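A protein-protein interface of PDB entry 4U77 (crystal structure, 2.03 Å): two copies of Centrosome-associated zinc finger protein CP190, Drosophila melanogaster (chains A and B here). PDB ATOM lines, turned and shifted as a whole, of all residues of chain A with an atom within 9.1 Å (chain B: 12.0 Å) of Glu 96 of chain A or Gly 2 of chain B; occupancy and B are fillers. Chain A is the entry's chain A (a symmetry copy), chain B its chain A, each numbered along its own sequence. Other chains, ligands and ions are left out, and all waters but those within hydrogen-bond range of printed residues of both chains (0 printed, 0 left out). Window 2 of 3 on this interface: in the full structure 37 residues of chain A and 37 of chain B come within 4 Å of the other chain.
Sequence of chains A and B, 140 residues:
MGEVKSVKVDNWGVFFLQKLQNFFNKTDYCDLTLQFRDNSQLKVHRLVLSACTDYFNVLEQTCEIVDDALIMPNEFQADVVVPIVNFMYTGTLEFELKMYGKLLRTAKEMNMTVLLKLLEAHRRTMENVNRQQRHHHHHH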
ATOM      1  N   ASP A  79     -24.630  -5.892  10.969  1.00  0.00           N
ATOM      2  CA  ASP A  79     -23.760  -4.927  11.649  1.00  0.00           C
ATOM      3  C   ASP A  79     -24.544  -3.704  12.148  1.00  0.00           C
ATOM      4  O   ASP A  79     -24.216  -3.153  13.196  1.00  0.00           O
ATOM      5  CB  ASP A  79     -22.610  -4.481  10.730  1.00  0.00           C
ATOM      6  CG  ASP A  79     -23.101  -3.858   9.446  1.00  0.00           C
ATOM      7  OD1 ASP A  79     -24.231  -4.190   9.020  1.00  0.00           O
ATOM      8  OD2 ASP A  79     -22.368  -3.028   8.871  1.00  0.00           O
ATOM      9  N   PRO A  83     -27.636  -4.234  16.425  1.00  0.00           N
ATOM     10  CA  PRO A  83     -27.686  -3.291  17.551  1.00  0.00           C
ATOM     11  C   PRO A  83     -28.936  -2.394  17.541  1.00  0.00           C
ATOM     12  O   PRO A  83     -29.376  -1.980  18.605  1.00  0.00           O
ATOM     13  CB  PRO A  83     -26.411  -2.446  17.370  1.00  0.00           C
ATOM     14  CG  PRO A  83     -25.999  -2.659  15.961  1.00  0.00           C
ATOM     15  CD  PRO A  83     -26.424  -4.044  15.606  1.00  0.00           C
ATOM     16  N   LEU A  93     -28.334   1.296  23.210  1.00  0.00           N
ATOM     17  CA  LEU A  93     -27.600   0.955  21.990  1.00  0.00           C
ATOM     18  C   LEU A  93     -26.157   0.579  22.315  1.00  0.00           C
ATOM     19  O   LEU A  93     -25.377   1.423  22.747  1.00  0.00           O
ATOM     20  CB  LEU A  93     -27.613   2.112  20.992  1.00  0.00           C
ATOM     21  CG  LEU A  93     -26.932   1.835  19.644  1.00  0.00           C
ATOM     22  CD1 LEU A  93     -27.882   1.106  18.694  1.00  0.00           C
ATOM     23  CD2 LEU A  93     -26.387   3.126  18.993  1.00  0.00           C
ATOM     24  N   GLU A  94     -25.808  -0.685  22.119  1.00  0.00           N
ATOM     25  CA  GLU A  94     -24.422  -1.129  22.294  1.00  0.00           C
ATOM     26  C   GLU A  94     -23.737  -1.106  20.944  1.00  0.00           C
ATOM     27  O   GLU A  94     -24.316  -1.551  19.955  1.00  0.00           O
ATOM     28  CB  GLU A  94     -24.357  -2.528  22.896  1.00  0.00           C
ATOM     29  CG  GLU A  94     -24.820  -2.585  24.334  1.00  0.00           C
ATOM     30  CD  GLU A  94     -24.802  -3.994  24.898  1.00  0.00           C
ATOM     31  OE1 GLU A  94     -25.133  -4.944  24.157  1.00  0.00           O
ATOM     32  OE2 GLU A  94     -24.451  -4.147  26.086  1.00  0.00           O
ATOM     33  N   PHE A  95     -22.522  -0.565  20.885  1.00  0.00           N
ATOM     34  CA  PHE A  95     -21.843  -0.415  19.601  1.00  0.00           C
ATOM     35  C   PHE A  95     -20.371  -0.079  19.728  1.00  0.00           C
ATOM     36  O   PHE A  95     -19.934   0.535  20.710  1.00  0.00           O
ATOM     37  CB  PHE A  95     -22.535   0.669  18.751  1.00  0.00           C
ATOM     38  CG  PHE A  95     -22.343   2.073  19.273  1.00  0.00           C
ATOM     39  CD1 PHE A  95     -21.487   2.954  18.639  1.00  0.00           C
ATOM     40  CD2 PHE A  95     -23.014   2.503  20.404  1.00  0.00           C
ATOM     41  CE1 PHE A  95     -21.311   4.239  19.122  1.00  0.00           C
ATOM     42  CE2 PHE A  95     -22.842   3.782  20.891  1.00  0.00           C
ATOM     43  CZ  PHE A  95     -21.989   4.649  20.256  1.00  0.00           C
ATOM     44  N   GLU A  96     -19.609  -0.477  18.715  1.00  0.00           N
ATOM     45  CA  GLU A  96     -18.210  -0.106  18.642  1.00  0.00           C
ATOM     46  C   GLU A  96     -18.165   1.292  18.045  1.00  0.00           C
ATOM     47  O   GLU A  96     -18.994   1.633  17.195  1.00  0.00           O
ATOM     48  CB  GLU A  96     -17.408  -1.107  17.812  1.00  0.00           C
ATOM     49  CG  GLU A  96     -17.184  -2.442  18.503  1.00  0.00           C
ATOM     50  CD  GLU A  96     -16.397  -3.428  17.648  1.00  0.00           C
ATOM     51  OE1 GLU A  96     -16.805  -4.608  17.567  1.00  0.00           O
ATOM     52  OE2 GLU A  96     -15.367  -3.022  17.065  1.00  0.00           O
ATOM     53  N   LEU A  97     -17.226   2.105  18.517  1.00  0.00           N
ATOM     54  CA  LEU A  97     -17.138   3.495  18.096  1.00  0.00           C
ATOM     55  C   LEU A  97     -17.048   3.625  16.593  1.00  0.00           C
ATOM     56  O   LEU A  97     -17.636   4.533  16.004  1.00  0.00           O
ATOM     57  CB  LEU A  97     -15.932   4.166  18.750  1.00  0.00           C
ATOM     58  CG  LEU A  97     -16.178   4.504  20.211  1.00  0.00           C
ATOM     59  CD1 LEU A  97     -14.981   5.250  20.754  1.00  0.00           C
ATOM     60  CD2 LEU A  97     -17.426   5.365  20.302  1.00  0.00           C
ATOM     61  N   LYS A  98     -16.309   2.712  15.968  1.00  0.00           N
ATOM     62  CA  LYS A  98     -16.113   2.779  14.526  1.00  0.00           C
ATOM     63  C   LYS A  98     -17.431   2.555  13.772  1.00  0.00           C
ATOM     64  O   LYS A  98     -17.521   2.849  12.576  1.00  0.00           O
ATOM     65  CB  LYS A  98     -15.054   1.768  14.075  1.00  0.00           C
ATOM     66  CG  LYS A  98     -15.422   0.297  14.288  1.00  0.00           C
ATOM     67  CD  LYS A  98     -14.456  -0.617  13.505  1.00  0.00           C
ATOM     68  CE  LYS A  98     -14.102  -1.884  14.282  1.00  0.00           C
ATOM     69  NZ  LYS A  98     -12.800  -2.484  13.838  1.00  0.00           N
ATOM     70  N   MET A  99     -18.445   2.057  14.476  1.00  0.00           N
ATOM     71  CA  MET A  99     -19.792   1.905  13.877  1.00  0.00           C
ATOM     72  C   MET A  99     -20.683   3.138  14.024  1.00  0.00           C
ATOM     73  O   MET A  99     -21.825   3.148  13.558  1.00  0.00           O
ATOM     74  CB  MET A  99     -20.525   0.712  14.497  1.00  0.00           C
ATOM     75  CG  MET A  99     -20.020  -0.668  14.032  1.00  0.00           C
ATOM     76  SD  MET A  99     -20.262  -0.911  12.252  1.00  0.00           S
ATOM     77  CE  MET A  99     -22.045  -0.705  12.115  1.00  0.00           C
ATOM     78  N   TYR A 100     -20.186   4.163  14.707  1.00  0.00           N
ATOM     79  CA  TYR A 100     -21.013   5.331  15.012  1.00  0.00           C
ATOM     80  C   TYR A 100     -21.618   5.973  13.772  1.00  0.00           C
ATOM     81  O   TYR A 100     -22.833   6.197  13.705  1.00  0.00           O
ATOM     82  CB  TYR A 100     -20.198   6.374  15.778  1.00  0.00           C
ATOM     83  CG  TYR A 100     -20.955   7.670  15.996  1.00  0.00           C
ATOM     84  CD1 TYR A 100     -21.846   7.803  17.052  1.00  0.00           C
ATOM     85  CD2 TYR A 100     -20.776   8.754  15.144  1.00  0.00           C
ATOM     86  CE1 TYR A 100     -22.542   8.982  17.256  1.00  0.00           C
ATOM     87  CE2 TYR A 100     -21.460   9.941  15.338  1.00  0.00           C
ATOM     88  CZ  TYR A 100     -22.341  10.048  16.395  1.00  0.00           C
ATOM     89  OH  TYR A 100     -23.019  11.221  16.596  1.00  0.00           O
ATOM     90  N   GLY A 101     -20.772   6.283  12.799  1.00  0.00           N
ATOM     91  CA  GLY A 101     -21.201   6.996  11.604  1.00  0.00           C
ATOM     92  C   GLY A 101     -22.227   6.200  10.817  1.00  0.00           C
ATOM     93  O   GLY A 101     -23.285   6.712  10.437  1.00  0.00           O
ATOM     94  N   LYS A 102     -21.930   4.929  10.578  1.00  0.00           N
ATOM     95  CA  LYS A 102     -22.863   4.078   9.839  1.00  0.00           C
ATOM     96  C   LYS A 102     -24.205   3.947  10.574  1.00  0.00           C
ATOM     97  O   LYS A 102     -25.255   3.958   9.940  1.00  0.00           O
ATOM     98  CB  LYS A 102     -22.262   2.698   9.590  1.00  0.00           C
ATOM     99  CG  LYS A 102     -22.855   2.009   8.366  1.00  0.00           C
ATOM    100  CD  LYS A 102     -22.196   0.665   8.084  1.00  0.00           C
ATOM    101  CE  LYS A 102     -22.906  -0.078   6.954  1.00  0.00           C
ATOM    102  NZ  LYS A 102     -22.265  -1.399   6.690  1.00  0.00           N
ATOM    103  N   LEU A 103     -24.170   3.834  11.901  1.00  0.00           N
ATOM    104  CA  LEU A 103     -25.411   3.708  12.670  1.00  0.00           C
ATOM    105  C   LEU A 103     -26.216   4.989  12.575  1.00  0.00           C
ATOM    106  O   LEU A 103     -27.429   4.954  12.387  1.00  0.00           O
ATOM    107  CB  LEU A 103     -25.124   3.370  14.130  1.00  0.00           C
ATOM    108  CG  LEU A 103     -24.769   1.899  14.335  1.00  0.00           C
ATOM    109  CD1 LEU A 103     -24.173   1.686  15.707  1.00  0.00           C
ATOM    110  CD2 LEU A 103     -26.007   1.008  14.131  1.00  0.00           C
ATOM    111  N   LEU A 119     -28.047   9.399  19.188  1.00  0.00           N
ATOM    112  CA  LEU A 119     -26.697   9.350  18.628  1.00  0.00           C
ATOM    113  C   LEU A 119     -26.125  10.740  18.476  1.00  0.00           C
ATOM    114  O   LEU A 119     -24.914  10.913  18.519  1.00  0.00           O
ATOM    115  CB  LEU A 119     -26.690   8.638  17.276  1.00  0.00           C
ATOM    116  CG  LEU A 119     -26.784   7.117  17.417  1.00  0.00           C
ATOM    117  CD1 LEU A 119     -27.064   6.472  16.073  1.00  0.00           C
ATOM    118  CD2 LEU A 119     -25.495   6.556  18.050  1.00  0.00           C
ATOM    119  N   GLY B   2     -11.949  -1.331  19.362  1.00  0.00           N
ATOM    120  CA  GLY B   2     -12.753  -2.537  19.276  1.00  0.00           C
ATOM    121  C   GLY B   2     -13.611  -2.723  20.513  1.00  0.00           C
ATOM    122  O   GLY B   2     -14.274  -3.752  20.691  1.00  0.00           O
ATOM    123  N   GLU B   3     -13.598  -1.716  21.376  1.00  0.00           N
ATOM    124  CA  GLU B   3     -14.352  -1.770  22.619  1.00  0.00           C
ATOM    125  C   GLU B   3     -15.794  -1.301  22.407  1.00  0.00           C
ATOM    126  O   GLU B   3     -16.030  -0.296  21.738  1.00  0.00           O
ATOM    127  CB  GLU B   3     -13.657  -0.925  23.687  1.00  0.00           C
ATOM    128  CG  GLU B   3     -14.543  -0.525  24.852  1.00  0.00           C
ATOM    129  CD  GLU B   3     -13.790   0.275  25.894  1.00  0.00           C
ATOM    130  OE1 GLU B   3     -12.543   0.172  25.934  1.00  0.00           O
ATOM    131  OE2 GLU B   3     -14.445   1.001  26.672  1.00  0.00           O
ATOM    132  N   VAL B   4     -16.744  -2.040  22.978  1.00  0.00           N
ATOM    133  CA  VAL B   4     -18.160  -1.732  22.841  1.00  0.00           C
ATOM    134  C   VAL B   4     -18.615  -0.728  23.896  1.00  0.00           C
ATOM    135  O   VAL B   4     -18.561  -0.999  25.095  1.00  0.00           O
ATOM    136  CB  VAL B   4     -19.031  -3.004  22.949  1.00  0.00           C
ATOM    137  CG1 VAL B   4     -20.486  -2.644  23.169  1.00  0.00           C
ATOM    138  CG2 VAL B   4     -18.877  -3.867  21.708  1.00  0.00           C
ATOM    139  N   LYS B   5     -19.048   0.441  23.440  1.00  0.00           N
ATOM    140  CA  LYS B   5     -19.626   1.437  24.334  1.00  0.00           C
ATOM    141  C   LYS B   5     -21.141   1.305  24.295  1.00  0.00           C
ATOM    142  O   LYS B   5     -21.673   0.486  23.546  1.00  0.00           O
ATOM    143  CB  LYS B   5     -19.192   2.842  23.922  1.00  0.00           C
ATOM    144  CG  LYS B   5     -17.770   2.916  23.371  1.00  0.00           C
ATOM    145  CD  LYS B   5     -16.708   3.005  24.463  1.00  0.00           C
ATOM    146  CE  LYS B   5     -15.350   3.348  23.857  1.00  0.00           C
ATOM    147  NZ  LYS B   5     -14.334   3.765  24.865  1.00  0.00           N
ATOM    148  N   SER B   6     -21.844   2.089  25.106  1.00  0.00           N
ATOM    149  CA  SER B   6     -23.293   2.142  24.994  1.00  0.00           C
ATOM    150  C   SER B   6     -23.856   3.465  25.504  1.00  0.00           C
ATOM    151  O   SER B   6     -23.326   4.067  26.437  1.00  0.00           O
ATOM    152  CB  SER B   6     -23.940   0.973  25.737  1.00  0.00           C
ATOM    153  OG  SER B   6     -23.889   1.169  27.133  1.00  0.00           O
ATOM    154  N   VAL B   7     -24.921   3.916  24.852  1.00  0.00           N
ATOM    155  CA  VAL B   7     -25.668   5.095  25.266  1.00  0.00           C
ATOM    156  C   VAL B   7     -27.101   4.639  25.454  1.00  0.00           C
ATOM    157  O   VAL B   7     -27.499   3.623  24.895  1.00  0.00           O
ATOM    158  CB  VAL B   7     -25.560   6.245  24.236  1.00  0.00           C
ATOM    159  CG1 VAL B   7     -24.214   6.953  24.355  1.00  0.00           C
ATOM    160  CG2 VAL B   7     -25.746   5.715  22.815  1.00  0.00           C
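The backbone NH (N) of Lys 5 of chain B is in hydrogen-bond range of the backbone carbonyl oxygen (O) of Phe 95 of chain A.
The backbone carbonyl oxygen (O) of Val 7 of chain B lies within hydrogen-bond range of the backbone NH (N) of Leu 93 of chain A, 3.0 Å away.
OE2 of Glu 3 of chain B is in salt-bridge range of NZ of Lys 5 of chain B (3.3 Å).
Among the printed residues, merely in contact across the chains: Leu 93 of chain A with Lys 5 of chain B (3.9 Å), Leu 93 of chain A with Ser 6 of chain B (3.1 Å), Glu 94 of chain A with Val 4 of chain B (3.9 Å), Glu 94 of chain A with Lys 5 of chain B (3.4 Å), Glu 94 of chain A with Ser 6 of chain B (3.9 Å), Phe 95 of chain A with Val 4 of chain B (3.6 Å), Phe 95 of chain A with Val 7 of chain B (3.98 Å), Glu 96 of chain A with Gly 2 of chain B (3.5 Å), Glu 96 of chain A with Glu 3 of chain B (3.8 Å), Glu 96 of chain A with Val 4 of chain B (3.9 Å) and Leu 97 of chain A with Lys 5 of chain B (3.7 Å).
Glu 96 of chain A touches three residues of chain B.
Gly 2 of chain B touches one residue of chain A.
Leu 97 of chain A touches one residue of chain B.
No residue of chain B comes within 4 Å of Lys 98 of chain A.
Met 99 of chain A touches none of the printed residues of chain B.
Printed residues of chain B within 4 Å of Glu 94 of chain A: Val 4 (3.9 Å), Lys 5 (3.4 Å) and Ser 6 (3.9 Å).
Of the printed residues of chain A, Val 7 of chain B touches Leu 93 (3.0 Å) and Phe 95 (3.98 Å).
Printed residues of chain A within 4 Å of Ser 6 of chain B: Leu 93 (3.1 Å) and Glu 94 (3.9 Å).
Of the printed residues of chain A, Glu 3 of chain B touches Glu 96 (3.8 Å).
Gly 101 of chain A touches none of the printed residues of chain B.
Asp 79 of chain A touches none of the printed residues of chain B.
The nearest residue of chain B that does not touch Glu 96 of chain A is Lys 5 of chain B (4.8 Å).
The nearest residue of chain A that does not touch Gly 2 of chain B is Lys 98 of chain A (5.2 Å).
Among the printed residues, no Asp or Glu carboxylate lies within 4 Å of a Lys or Arg side-chain nitrogen of the other chain.
No position is printed for both chains.
Of the 13 pairs that touch across the chains among the printed residues, none has its exchanged pair printed and touching as well.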
